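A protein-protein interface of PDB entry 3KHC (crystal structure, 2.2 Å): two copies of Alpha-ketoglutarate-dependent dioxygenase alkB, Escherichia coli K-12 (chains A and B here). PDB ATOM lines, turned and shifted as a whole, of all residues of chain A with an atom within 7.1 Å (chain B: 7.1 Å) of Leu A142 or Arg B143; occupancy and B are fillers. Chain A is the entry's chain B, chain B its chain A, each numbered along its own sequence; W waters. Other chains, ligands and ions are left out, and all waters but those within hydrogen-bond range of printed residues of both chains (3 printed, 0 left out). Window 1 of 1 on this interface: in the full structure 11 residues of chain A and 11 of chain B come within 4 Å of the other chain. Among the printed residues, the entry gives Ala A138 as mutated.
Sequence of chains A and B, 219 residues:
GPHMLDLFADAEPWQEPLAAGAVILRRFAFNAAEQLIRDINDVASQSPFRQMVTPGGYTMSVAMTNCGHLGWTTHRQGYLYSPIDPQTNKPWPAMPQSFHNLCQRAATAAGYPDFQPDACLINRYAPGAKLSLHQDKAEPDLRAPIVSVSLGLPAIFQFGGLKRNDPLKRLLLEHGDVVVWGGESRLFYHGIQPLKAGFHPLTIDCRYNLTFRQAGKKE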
ATOM      1  N   ASP A 136     -21.005  -8.914   1.718  1.00  0.00           N
ATOM      2  CA  ASP A 136     -21.942  -7.864   1.328  1.00  0.00           C
ATOM      3  C   ASP A 136     -21.382  -7.181   0.100  1.00  0.00           C
ATOM      4  O   ASP A 136     -20.551  -6.266   0.210  1.00  0.00           O
ATOM      5  CB  ASP A 136     -22.162  -6.847   2.449  1.00  0.00           C
ATOM      6  CG  ASP A 136     -22.950  -7.419   3.598  1.00  0.00           C
ATOM      7  OD1 ASP A 136     -23.045  -8.661   3.671  1.00  0.00           O
ATOM      8  OD2 ASP A 136     -23.471  -6.634   4.421  1.00  0.00           O
ATOM      9  N   LYS A 137     -21.821  -7.635  -1.069  1.00  0.00           N
ATOM     10  CA  LYS A 137     -21.313  -7.102  -2.324  1.00  0.00           C
ATOM     11  C   LYS A 137     -22.409  -6.636  -3.281  1.00  0.00           C
ATOM     12  O   LYS A 137     -22.123  -6.277  -4.422  1.00  0.00           O
ATOM     13  CB  LYS A 137     -20.366  -8.099  -2.995  1.00  0.00           C
ATOM     14  CG  LYS A 137     -21.011  -9.374  -3.494  1.00  0.00           C
ATOM     15  CD  LYS A 137     -20.013 -10.175  -4.310  1.00  0.00           C
ATOM     16  CE  LYS A 137     -20.454 -11.610  -4.481  1.00  0.00           C
ATOM     17  NZ  LYS A 137     -19.463 -12.359  -5.315  1.00  0.00           N
ATOM     18  N   ALA A 138     -23.650  -6.586  -2.801  1.00  0.00           N
ATOM     19  CA  ALA A 138     -24.764  -6.076  -3.610  1.00  0.00           C
ATOM     20  C   ALA A 138     -24.835  -4.533  -3.677  1.00  0.00           C
ATOM     21  O   ALA A 138     -25.724  -3.980  -4.324  1.00  0.00           O
ATOM     22  CB  ALA A 138     -26.086  -6.661  -3.124  1.00  0.00           C
ATOM     23  N   GLU A 139     -23.900  -3.857  -3.007  1.00  0.00           N
ATOM     24  CA  GLU A 139     -23.890  -2.398  -2.914  1.00  0.00           C
ATOM     25  C   GLU A 139     -22.901  -1.807  -3.909  1.00  0.00           C
ATOM     26  O   GLU A 139     -21.738  -2.221  -3.944  1.00  0.00           O
ATOM     27  CB  GLU A 139     -23.536  -1.933  -1.493  1.00  0.00           C
ATOM     28  CG  GLU A 139     -24.494  -2.393  -0.408  1.00  0.00           C
ATOM     29  CD  GLU A 139     -24.276  -3.848   0.024  1.00  0.00           C
ATOM     30  OE1 GLU A 139     -25.262  -4.482   0.443  1.00  0.00           O
ATOM     31  OE2 GLU A 139     -23.139  -4.365  -0.054  1.00  0.00           O
ATOM     32  N   PRO A 140     -23.357  -0.832  -4.722  1.00  0.00           N
ATOM     33  CA  PRO A 140     -22.520  -0.274  -5.785  1.00  0.00           C
ATOM     34  C   PRO A 140     -21.376   0.623  -5.295  1.00  0.00           C
ATOM     35  O   PRO A 140     -20.356   0.739  -5.988  1.00  0.00           O
ATOM     36  CB  PRO A 140     -23.514   0.529  -6.626  1.00  0.00           C
ATOM     37  CG  PRO A 140     -24.626   0.833  -5.703  1.00  0.00           C
ATOM     38  CD  PRO A 140     -24.742  -0.342  -4.806  1.00  0.00           C
ATOM     39  N   ASP A 141     -21.540   1.248  -4.129  1.00  0.00           N
ATOM     40  CA  ASP A 141     -20.527   2.156  -3.588  1.00  0.00           C
ATOM     41  C   ASP A 141     -19.801   1.567  -2.369  1.00  0.00           C
ATOM     42  O   ASP A 141     -20.255   1.702  -1.228  1.00  0.00           O
ATOM     43  CB  ASP A 141     -21.148   3.512  -3.245  1.00  0.00           C
ATOM     44  CG  ASP A 141     -20.108   4.566  -2.895  1.00  0.00           C
ATOM     45  OD1 ASP A 141     -18.891   4.256  -2.867  1.00  0.00           O
ATOM     46  OD2 ASP A 141     -20.510   5.717  -2.636  1.00  0.00           O
ATOM     47  N   LEU A 142     -18.657   0.938  -2.627  1.00  0.00           N
ATOM     48  CA  LEU A 142     -17.909   0.206  -1.600  1.00  0.00           C
ATOM     49  C   LEU A 142     -17.172   1.070  -0.579  1.00  0.00           C
ATOM     50  O   LEU A 142     -16.567   0.535   0.355  1.00  0.00           O
ATOM     51  CB  LEU A 142     -16.943  -0.796  -2.246  1.00  0.00           C
ATOM     52  CG  LEU A 142     -17.648  -1.886  -3.058  1.00  0.00           C
ATOM     53  CD1 LEU A 142     -16.652  -2.714  -3.860  1.00  0.00           C
ATOM     54  CD2 LEU A 142     -18.514  -2.757  -2.137  1.00  0.00           C
ATOM     55  N   ARG A 143     -17.222   2.390  -0.740  1.00  0.00           N
ATOM     56  CA  ARG A 143     -16.589   3.289   0.216  1.00  0.00           C
ATOM     57  C   ARG A 143     -17.333   3.303   1.550  1.00  0.00           C
ATOM     58  O   ARG A 143     -16.725   3.550   2.595  1.00  0.00           O
ATOM     59  CB  ARG A 143     -16.494   4.713  -0.332  1.00  0.00           C
ATOM     60  CG  ARG A 143     -15.552   4.876  -1.535  1.00  0.00           C
ATOM     61  CD  ARG A 143     -15.696   6.262  -2.155  1.00  0.00           C
ATOM     62  NE  ARG A 143     -17.049   6.503  -2.671  1.00  0.00           N
ATOM     63  CZ  ARG A 143     -17.489   7.679  -3.115  1.00  0.00           C
ATOM     64  NH1 ARG A 143     -16.681   8.746  -3.119  1.00  0.00           N
ATOM     65  NH2 ARG A 143     -18.740   7.793  -3.565  1.00  0.00           N
ATOM     66  N   ALA A 144     -18.642   3.046   1.509  1.00  0.00           N
ATOM     67  CA  ALA A 144     -19.470   3.162   2.693  1.00  0.00           C
ATOM     68  C   ALA A 144     -19.323   1.922   3.561  1.00  0.00           C
ATOM     69  O   ALA A 144     -19.335   0.800   3.045  1.00  0.00           O
ATOM     70  CB  ALA A 144     -20.926   3.381   2.316  1.00  0.00           C
ATOM     71  N   PRO A 145     -19.180   2.117   4.887  1.00  0.00           N
ATOM     72  CA  PRO A 145     -18.994   0.979   5.785  1.00  0.00           C
ATOM     73  C   PRO A 145     -20.281   0.173   6.017  1.00  0.00           C
ATOM     74  O   PRO A 145     -21.368   0.566   5.578  1.00  0.00           O
ATOM     75  CB  PRO A 145     -18.538   1.647   7.085  1.00  0.00           C
ATOM     76  CG  PRO A 145     -19.216   2.971   7.059  1.00  0.00           C
ATOM     77  CD  PRO A 145     -19.157   3.399   5.620  1.00  0.00           C
ATOM     78  N   LEU A 162     -11.064 -12.136   2.702  1.00  0.00           N
ATOM     79  CA  LEU A 162     -11.497 -11.750   1.350  1.00  0.00           C
ATOM     80  C   LEU A 162     -11.830 -12.996   0.516  1.00  0.00           C
ATOM     81  O   LEU A 162     -12.662 -12.941  -0.392  1.00  0.00           O
ATOM     82  CB  LEU A 162     -10.431 -10.913   0.627  1.00  0.00           C
ATOM     83  CG  LEU A 162     -10.856  -9.606  -0.069  1.00  0.00           C
ATOM     84  CD1 LEU A 162      -9.918  -9.284  -1.251  1.00  0.00           C
ATOM     85  CD2 LEU A 162     -12.320  -9.585  -0.530  1.00  0.00           C
ATOM     86  N   GLY A 182     -15.316  -2.041   6.839  1.00  0.00           N
ATOM     87  CA  GLY A 182     -15.189  -1.203   5.659  1.00  0.00           C
ATOM     88  C   GLY A 182     -13.747  -0.971   5.240  1.00  0.00           C
ATOM     89  O   GLY A 182     -12.811  -1.536   5.824  1.00  0.00           O
ATOM     90  N   GLY A 183     -13.567  -0.127   4.230  1.00  0.00           N
ATOM     91  CA  GLY A 183     -12.245   0.101   3.637  1.00  0.00           C
ATOM     92  C   GLY A 183     -11.677  -1.255   3.276  1.00  0.00           C
ATOM     93  O   GLY A 183     -12.361  -2.079   2.670  1.00  0.00           O
ATOM     94  N   GLU A 184     -10.450  -1.514   3.700  1.00  0.00           N
ATOM     95  CA  GLU A 184      -9.793  -2.792   3.416  1.00  0.00           C
ATOM     96  C   GLU A 184     -10.614  -4.057   3.735  1.00  0.00           C
ATOM     97  O   GLU A 184     -10.490  -5.057   3.022  1.00  0.00           O
ATOM     98  CB  GLU A 184      -8.428  -2.847   4.102  1.00  0.00           C
ATOM     99  CG  GLU A 184      -7.382  -1.973   3.424  1.00  0.00           C
ATOM    100  CD  GLU A 184      -6.806  -2.605   2.168  1.00  0.00           C
ATOM    101  OE1 GLU A 184      -5.961  -3.519   2.308  1.00  0.00           O
ATOM    102  OE2 GLU A 184      -7.172  -2.177   1.042  1.00  0.00           O
ATOM    103  N   SER A 185     -11.448  -4.004   4.780  1.00  0.00           N
ATOM    104  CA  SER A 185     -12.281  -5.147   5.190  1.00  0.00           C
ATOM    105  C   SER A 185     -13.737  -5.113   4.677  1.00  0.00           C
ATOM    106  O   SER A 185     -14.566  -5.958   5.058  1.00  0.00           O
ATOM    107  CB  SER A 185     -12.266  -5.316   6.728  1.00  0.00           C
ATOM    108  OG  SER A 185     -12.854  -4.186   7.366  1.00  0.00           O
ATOM    109  N   ARG A 186     -14.050  -4.154   3.814  1.00  0.00           N
ATOM    110  CA  ARG A 186     -15.413  -3.992   3.309  1.00  0.00           C
ATOM    111  C   ARG A 186     -16.034  -5.250   2.673  1.00  0.00           C
ATOM    112  O   ARG A 186     -17.228  -5.490   2.827  1.00  0.00           O
ATOM    113  CB  ARG A 186     -15.490  -2.804   2.350  1.00  0.00           C
ATOM    114  CG  ARG A 186     -16.865  -2.541   1.755  1.00  0.00           C
ATOM    115  CD  ARG A 186     -17.914  -2.273   2.825  1.00  0.00           C
ATOM    116  NE  ARG A 186     -19.216  -1.900   2.262  1.00  0.00           N
ATOM    117  CZ  ARG A 186     -20.051  -2.740   1.651  1.00  0.00           C
ATOM    118  NH1 ARG A 186     -19.724  -4.022   1.493  1.00  0.00           N
ATOM    119  NH2 ARG A 186     -21.209  -2.287   1.184  1.00  0.00           N
ATOM    120  N   LEU A 187     -15.239  -6.034   1.962  1.00  0.00           N
ATOM    121  CA  LEU A 187     -15.755  -7.214   1.267  1.00  0.00           C
ATOM    122  C   LEU A 187     -15.418  -8.535   1.977  1.00  0.00           C
ATOM    123  O   LEU A 187     -15.543  -9.614   1.389  1.00  0.00           O
ATOM    124  CB  LEU A 187     -15.266  -7.238  -0.193  1.00  0.00           C
ATOM    125  CG  LEU A 187     -15.911  -6.238  -1.165  1.00  0.00           C
ATOM    126  CD1 LEU A 187     -15.135  -6.120  -2.510  1.00  0.00           C
ATOM    127  CD2 LEU A 187     -17.363  -6.587  -1.418  1.00  0.00           C
ATOM    128  N   PHE A 188     -15.002  -8.450   3.239  1.00  0.00           N
ATOM    129  CA  PHE A 188     -14.647  -9.635   4.003  1.00  0.00           C
ATOM    130  C   PHE A 188     -15.869 -10.530   4.204  1.00  0.00           C
ATOM    131  O   PHE A 188     -16.994 -10.045   4.375  1.00  0.00           O
ATOM    132  CB  PHE A 188     -14.019  -9.261   5.360  1.00  0.00           C
ATOM    133  CG  PHE A 188     -12.559  -8.861   5.290  1.00  0.00           C
ATOM    134  CD1 PHE A 188     -11.775  -8.878   6.438  1.00  0.00           C
ATOM    135  CD2 PHE A 188     -11.968  -8.454   4.083  1.00  0.00           C
ATOM    136  CE1 PHE A 188     -10.419  -8.497   6.399  1.00  0.00           C
ATOM    137  CE2 PHE A 188     -10.614  -8.086   4.028  1.00  0.00           C
ATOM    138  CZ  PHE A 188      -9.840  -8.105   5.190  1.00  0.00           C
ATOM    139  N   GLN A 214     -25.060   1.968   3.005  1.00  0.00           N
ATOM    140  CA  GLN A 214     -25.412   2.844   1.894  1.00  0.00           C
ATOM    141  C   GLN A 214     -25.571   1.877   0.726  1.00  0.00           C
ATOM    142  O   GLN A 214     -24.603   1.270   0.281  1.00  0.00           O
ATOM    143  CB  GLN A 214     -24.350   3.930   1.626  1.00  0.00           C
ATOM    144  CG  GLN A 214     -24.654   4.849   0.427  1.00  0.00           C
ATOM    145  CD  GLN A 214     -23.392   5.458  -0.226  1.00  0.00           C
ATOM    146  OE1 GLN A 214     -23.185   5.327  -1.436  1.00  0.00           O
ATOM    147  NE2 GLN A 214     -22.558   6.118   0.572  1.00  0.00           N
ATOM    148  N   TYR B 112      -3.028   6.892   0.399  1.00  0.00           N
ATOM    149  CA  TYR B 112      -3.637   5.663  -0.094  1.00  0.00           C
ATOM    150  C   TYR B 112      -2.596   4.538  -0.183  1.00  0.00           C
ATOM    151  O   TYR B 112      -2.147   4.195  -1.281  1.00  0.00           O
ATOM    152  CB  TYR B 112      -4.301   5.905  -1.450  1.00  0.00           C
ATOM    153  CG  TYR B 112      -5.369   6.969  -1.413  1.00  0.00           C
ATOM    154  CD1 TYR B 112      -5.071   8.292  -1.738  1.00  0.00           C
ATOM    155  CD2 TYR B 112      -6.690   6.651  -1.068  1.00  0.00           C
ATOM    156  CE1 TYR B 112      -6.056   9.276  -1.717  1.00  0.00           C
ATOM    157  CE2 TYR B 112      -7.678   7.625  -1.035  1.00  0.00           C
ATOM    158  CZ  TYR B 112      -7.354   8.937  -1.363  1.00  0.00           C
ATOM    159  OH  TYR B 112      -8.327   9.910  -1.335  1.00  0.00           O
ATOM    160  N   PHE B 115      -3.243   1.124  -2.684  1.00  0.00           N
ATOM    161  CA  PHE B 115      -3.644   1.228  -4.082  1.00  0.00           C
ATOM    162  C   PHE B 115      -2.878   0.227  -4.937  1.00  0.00           C
ATOM    163  O   PHE B 115      -1.645   0.182  -4.925  1.00  0.00           O
ATOM    164  CB  PHE B 115      -3.454   2.664  -4.603  1.00  0.00           C
ATOM    165  CG  PHE B 115      -3.984   2.896  -6.015  1.00  0.00           C
ATOM    166  CD1 PHE B 115      -5.125   2.242  -6.477  1.00  0.00           C
ATOM    167  CD2 PHE B 115      -3.349   3.798  -6.870  1.00  0.00           C
ATOM    168  CE1 PHE B 115      -5.607   2.471  -7.769  1.00  0.00           C
ATOM    169  CE2 PHE B 115      -3.830   4.034  -8.162  1.00  0.00           C
ATOM    170  CZ  PHE B 115      -4.958   3.366  -8.612  1.00  0.00           C
ATOM    171  N   PRO B 140     -16.024  -0.069 -10.808  1.00  0.00           N
ATOM    172  CA  PRO B 140     -16.969  -0.589  -9.820  1.00  0.00           C
ATOM    173  C   PRO B 140     -16.506  -0.463  -8.364  1.00  0.00           C
ATOM    174  O   PRO B 140     -17.347  -0.426  -7.475  1.00  0.00           O
ATOM    175  CB  PRO B 140     -17.114  -2.064 -10.217  1.00  0.00           C
ATOM    176  CG  PRO B 140     -15.827  -2.401 -10.839  1.00  0.00           C
ATOM    177  CD  PRO B 140     -15.386  -1.157 -11.577  1.00  0.00           C
ATOM    178  N   ASP B 141     -15.198  -0.413  -8.126  1.00  0.00           N
ATOM    179  CA  ASP B 141     -14.648  -0.313  -6.772  1.00  0.00           C
ATOM    180  C   ASP B 141     -14.170   1.119  -6.501  1.00  0.00           C
ATOM    181  O   ASP B 141     -13.044   1.491  -6.840  1.00  0.00           O
ATOM    182  CB  ASP B 141     -13.512  -1.333  -6.570  1.00  0.00           C
ATOM    183  CG  ASP B 141     -13.143  -1.546  -5.090  1.00  0.00           C
ATOM    184  OD1 ASP B 141     -13.567  -0.739  -4.221  1.00  0.00           O
ATOM    185  OD2 ASP B 141     -12.425  -2.536  -4.793  1.00  0.00           O
ATOM    186  N   LEU B 142     -15.040   1.914  -5.886  1.00  0.00           N
ATOM    187  CA  LEU B 142     -14.777   3.328  -5.664  1.00  0.00           C
ATOM    188  C   LEU B 142     -13.812   3.624  -4.512  1.00  0.00           C
ATOM    189  O   LEU B 142     -13.448   4.789  -4.300  1.00  0.00           O
ATOM    190  CB  LEU B 142     -16.095   4.102  -5.484  1.00  0.00           C
ATOM    191  CG  LEU B 142     -17.056   4.147  -6.680  1.00  0.00           C
ATOM    192  CD1 LEU B 142     -18.333   4.871  -6.310  1.00  0.00           C
ATOM    193  CD2 LEU B 142     -16.419   4.799  -7.918  1.00  0.00           C
ATOM    194  N   ARG B 143     -13.392   2.591  -3.772  1.00  0.00           N
ATOM    195  CA  ARG B 143     -12.383   2.781  -2.708  1.00  0.00           C
ATOM    196  C   ARG B 143     -10.984   3.114  -3.269  1.00  0.00           C
ATOM    197  O   ARG B 143     -10.165   3.741  -2.595  1.00  0.00           O
ATOM    198  CB  ARG B 143     -12.286   1.560  -1.784  1.00  0.00           C
ATOM    199  CG  ARG B 143     -13.597   1.126  -1.134  1.00  0.00           C
ATOM    200  CD  ARG B 143     -13.468  -0.250  -0.478  1.00  0.00           C
ATOM    201  NE  ARG B 143     -12.994  -1.280  -1.409  1.00  0.00           N
ATOM    202  CZ  ARG B 143     -12.718  -2.540  -1.067  1.00  0.00           C
ATOM    203  NH1 ARG B 143     -12.873  -2.955   0.189  1.00  0.00           N
ATOM    204  NH2 ARG B 143     -12.285  -3.391  -1.988  1.00  0.00           N
ATOM    205  N   ALA B 144     -10.708   2.671  -4.491  1.00  0.00           N
ATOM    206  CA  ALA B 144      -9.423   2.951  -5.127  1.00  0.00           C
ATOM    207  C   ALA B 144      -9.373   4.394  -5.616  1.00  0.00           C
ATOM    208  O   ALA B 144     -10.320   4.861  -6.253  1.00  0.00           O
ATOM    209  CB  ALA B 144      -9.166   1.988  -6.272  1.00  0.00           C
ATOM    210  N   PRO B 145      -8.283   5.111  -5.308  1.00  0.00           N
ATOM    211  CA  PRO B 145      -8.136   6.482  -5.787  1.00  0.00           C
ATOM    212  C   PRO B 145      -7.765   6.550  -7.279  1.00  0.00           C
ATOM    213  O   PRO B 145      -7.479   5.520  -7.899  1.00  0.00           O
ATOM    214  CB  PRO B 145      -6.973   7.010  -4.945  1.00  0.00           C
ATOM    215  CG  PRO B 145      -6.126   5.806  -4.729  1.00  0.00           C
ATOM    216  CD  PRO B 145      -7.098   4.668  -4.551  1.00  0.00           C
ATOM    217  N   ILE B 146      -7.802   7.755  -7.840  1.00  0.00           N
ATOM    218  CA  ILE B 146      -7.252   8.030  -9.179  1.00  0.00           C
ATOM    219  C   ILE B 146      -5.889   8.685  -8.982  1.00  0.00           C
ATOM    220  O   ILE B 146      -5.767   9.634  -8.205  1.00  0.00           O
ATOM    221  CB  ILE B 146      -8.144   9.015 -10.011  1.00  0.00           C
ATOM    222  CG1 ILE B 146      -9.610   8.542 -10.078  1.00  0.00           C
ATOM    223  CG2 ILE B 146      -7.547   9.255 -11.417  1.00  0.00           C
ATOM    224  CD1 ILE B 146      -9.829   7.224 -10.814  1.00  0.00           C
ATOM    225  N   TRP B 181      -6.756  11.819  -6.256  1.00  0.00           N
ATOM    226  CA  TRP B 181      -8.019  12.023  -5.566  1.00  0.00           C
ATOM    227  C   TRP B 181      -8.732  10.701  -5.301  1.00  0.00           C
ATOM    228  O   TRP B 181      -8.503   9.717  -6.003  1.00  0.00           O
ATOM    229  CB  TRP B 181      -8.904  13.060  -6.269  1.00  0.00           C
ATOM    230  CG  TRP B 181      -9.407  12.724  -7.637  1.00  0.00           C
ATOM    231  CD1 TRP B 181     -10.639  12.244  -7.953  1.00  0.00           C
ATOM    232  CD2 TRP B 181      -8.704  12.881  -8.883  1.00  0.00           C
ATOM    233  NE1 TRP B 181     -10.752  12.081  -9.317  1.00  0.00           N
ATOM    234  CE2 TRP B 181      -9.580  12.471  -9.912  1.00  0.00           C
ATOM    235  CE3 TRP B 181      -7.421  13.337  -9.229  1.00  0.00           C
ATOM    236  CZ2 TRP B 181      -9.215  12.498 -11.278  1.00  0.00           C
ATOM    237  CZ3 TRP B 181      -7.057  13.370 -10.597  1.00  0.00           C
ATOM    238  CH2 TRP B 181      -7.949  12.946 -11.593  1.00  0.00           C
ATOM    239  N   GLY B 182      -9.573  10.691  -4.271  1.00  0.00           N
ATOM    240  CA  GLY B 182     -10.280   9.487  -3.842  1.00  0.00           C
ATOM    241  C   GLY B 182     -11.063   9.755  -2.566  1.00  0.00           C
ATOM    242  O   GLY B 182     -11.127  10.895  -2.097  1.00  0.00           O
ATOM    243  N   GLY B 183     -11.646   8.705  -1.984  1.00  0.00           N
ATOM    244  CA  GLY B 183     -12.522   8.868  -0.822  1.00  0.00           C
ATOM    245  C   GLY B 183     -13.652   9.835  -1.157  1.00  0.00           C
ATOM    246  O   GLY B 183     -14.381   9.629  -2.126  1.00  0.00           O
ATOM    247  N   ARG B 186     -13.716  11.222  -4.677  1.00  0.00           N
ATOM    248  CA  ARG B 186     -13.439  10.181  -5.690  1.00  0.00           C
ATOM    249  C   ARG B 186     -14.190  10.369  -7.006  1.00  0.00           C
ATOM    250  O   ARG B 186     -13.629  10.140  -8.091  1.00  0.00           O
ATOM    251  CB  ARG B 186     -13.638   8.757  -5.148  1.00  0.00           C
ATOM    252  CG  ARG B 186     -13.530   7.625  -6.201  1.00  0.00           C
ATOM    253  CD  ARG B 186     -12.144   7.508  -6.863  1.00  0.00           C
ATOM    254  NE  ARG B 186     -12.086   6.374  -7.794  1.00  0.00           N
ATOM    255  CZ  ARG B 186     -12.616   6.351  -9.021  1.00  0.00           C
ATOM    256  NH1 ARG B 186     -13.263   7.403  -9.513  1.00  0.00           N
ATOM    257  NH2 ARG B 186     -12.512   5.257  -9.758  1.00  0.00           N
ATOM    258  N   GLN B 214      -7.784   1.462 -10.399  1.00  0.00           N
ATOM    259  CA  GLN B 214      -8.296   0.112 -10.202  1.00  0.00           C
ATOM    260  C   GLN B 214      -9.637   0.037 -10.932  1.00  0.00           C
ATOM    261  O   GLN B 214     -10.628   0.631 -10.507  1.00  0.00           O
ATOM    262  CB  GLN B 214      -8.446  -0.254  -8.719  1.00  0.00           C
ATOM    263  CG  GLN B 214      -8.872  -1.705  -8.499  1.00  0.00           C
ATOM    264  CD  GLN B 214      -9.462  -1.965  -7.117  1.00  0.00           C
ATOM    265  OE1 GLN B 214     -10.462  -2.673  -6.983  1.00  0.00           O
ATOM    266  NE2 GLN B 214      -8.839  -1.403  -6.085  1.00  0.00           N
ATOM    267  N   LYS B 217     -11.710  -5.863 -10.030  1.00  0.00           N
ATOM    268  CA  LYS B 217     -11.879  -6.229  -8.617  1.00  0.00           C
ATOM    269  C   LYS B 217     -10.544  -6.406  -7.883  1.00  0.00           C
ATOM    270  O   LYS B 217      -9.583  -6.935  -8.444  1.00  0.00           O
ATOM    271  CB  LYS B 217     -12.735  -7.497  -8.474  1.00  0.00           C
ATOM    272  CG  LYS B 217     -14.054  -7.504  -9.264  1.00  0.00           C
ATOM    273  CD  LYS B 217     -14.945  -6.290  -8.985  1.00  0.00           C
ATOM    274  CE  LYS B 217     -16.350  -6.517  -9.543  1.00  0.00           C
ATOM    275  NZ  LYS B 217     -17.383  -5.621  -8.945  1.00  0.00           N
ATOM    276  N   LYS B 218     -10.499  -5.961  -6.626  1.00  0.00           N
ATOM    277  CA  LYS B 218      -9.274  -6.011  -5.822  1.00  0.00           C
ATOM    278  C   LYS B 218      -9.085  -7.373  -5.150  1.00  0.00           C
ATOM    279  O   LYS B 218     -10.059  -8.031  -4.775  1.00  0.00           O
ATOM    280  CB  LYS B 218      -9.273  -4.899  -4.767  1.00  0.00           C
ATOM    281  CG  LYS B 218      -7.907  -4.618  -4.163  1.00  0.00           C
ATOM    282  CD  LYS B 218      -8.000  -3.756  -2.909  1.00  0.00           C
ATOM    283  CE  LYS B 218      -6.679  -3.049  -2.624  1.00  0.00           C
ATOM    284  NZ  LYS B 218      -5.495  -3.915  -2.890  1.00  0.00           N
ATOM    285  N   GLU B 219      -7.821  -7.774  -5.002  1.00  0.00           N
ATOM    286  CA  GLU B 219      -7.432  -9.014  -4.325  1.00  0.00           C
ATOM    287  C   GLU B 219      -6.836  -8.769  -2.939  1.00  0.00           C
ATOM    288  O   GLU B 219      -6.754  -7.628  -2.470  1.00  0.00           O
ATOM    289  CB  GLU B 219      -6.434  -9.788  -5.180  1.00  0.00           C
ATOM    290  CG  GLU B 219      -7.053 -10.388  -6.425  1.00  0.00           C
ATOM    291  CD  GLU B 219      -6.048 -11.101  -7.284  1.00  0.00           C
ATOM    292  OE1 GLU B 219      -4.944 -10.554  -7.477  1.00  0.00           O
ATOM    293  OE2 GLU B 219      -6.365 -12.208  -7.771  1.00  0.00           O
HETATM  294  O   HOH W   1     -16.862  11.532  -4.484  1.00  0.00           O
HETATM  295  O   HOH W   2     -12.231  -5.850   1.152  1.00  0.00           O
HETATM  296  O   HOH W   3     -17.511   0.889  -5.242  1.00  0.00           O
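NH1 of Arg B143 is in hydrogen-bond range of O of Gly A183 (2.7 Å).
The backbone carbonyl oxygen (O) of Gly B183 sits at hydrogen-bond distance from the guanidinium group (NH1) of Arg A143.
The side-chain carboxylate (OD1) of Asp B141 is in salt-bridge range of the guanidinium group (NE) of Arg B143, at 2.9 Å.
O of Ala B144 is in hydrogen-bond range of NE of Arg B186 (2.8 Å).
O of Asp A136 sits at hydrogen-bond distance from NH1 of Arg A186 (2.7 Å).
The guanidinium group of Arg A186 is in salt-bridge range of the side-chain carboxylate of Glu A139 (3.1 Å).
The side-chain carboxylate (OD2) of Asp A141 is in salt-bridge range of the guanidinium group (NH2) of Arg A143.
The backbone carbonyl oxygen of Ala A144 sits at hydrogen-bond distance from the guanidinium group of Arg A186 (2.8 Å).
Among the printed residues, pairs that only touch across the chains: Leu A142 with Arg B143, Arg A186 with Arg B143, Arg A143 with Leu B142, Asp A141 with Leu B142, Leu A162 with Glu B219, Pro A140 with Pro B140, Arg A143 with Arg B186, Leu A142 with Asp B141, Leu A162 with Lys B218, Glu A184 with Lys B218, Arg A143 with Arg B143 and Leu A187 with Arg B143.
Of the printed residues of chain B, Arg A143 touches Leu B142, Arg B143, Gly B183 and Arg B186.
Of the printed residues of chain B, Glu A184 touches Lys B218 (3.8 Å).
Of the printed residues of chain B, Arg A186 touches Arg B143 (3.4 Å).
Phe B115 touches none of the printed residues of chain A.
Printed residues of chain A within 4 Å of Leu B142: Asp A141 (3.5 Å) and Arg A143 (3.4 Å).
The nearest residue of chain B that does not touch Leu A142 is Pro B140 (4.3 Å).
The nearest printed residue of chain B that does not touch Leu A187 is Asp B141 (5.0 Å).
Of the 17 printed residues of chain B, 8 touch a printed residue of chain A.
Printed residues of chain A that touch a printed residue of chain B: Pro A140, Asp A141, Leu A142, Arg A143, Leu A162, Gly A183, Glu A184, Arg A186 and Leu A187.
Hydrophobic or aromatic side chains of chain A within 4 Å of the printed part of chain B: Leu A142, Leu A162 and Leu A187.
Among the printed residues, 14 pairs touch across the chains.
Among the printed residues, no Asp or Glu carboxylate lies within 4 Å of a Lys or Arg side-chain nitrogen of the other chain.
Asp A141 touches Leu B142, and with the chains exchanged Leu A142 touches Asp B141.
Arg B143 touches its own counterpart, Arg A143.
Arg A143 touches Gly B183, and with the chains exchanged Gly A183 touches Arg B143.
Arg A143 touches Arg B186, and with the chains exchanged Arg A186 touches Arg B143.
Of the 14 pairs that touch across the chains among the printed residues, 10 have their exchanged pair printed and touching as well.
Water W3 lies within hydrogen-bond range of the backbone carbonyl oxygen (O) of Pro B140, the backbone NH (N) of Leu B142, the backbone NH (N) of Leu A142 and the backbone carbonyl oxygen (O) of Pro A140.
Water W2 lies within hydrogen-bond range of O of Glu A184, NH1 of Arg B143 and N of Leu A187.
Water W1 bridges the guanidinium group of Arg A143 (3.1 Å) and the backbone NH of Arg B186 (3.2 Å).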
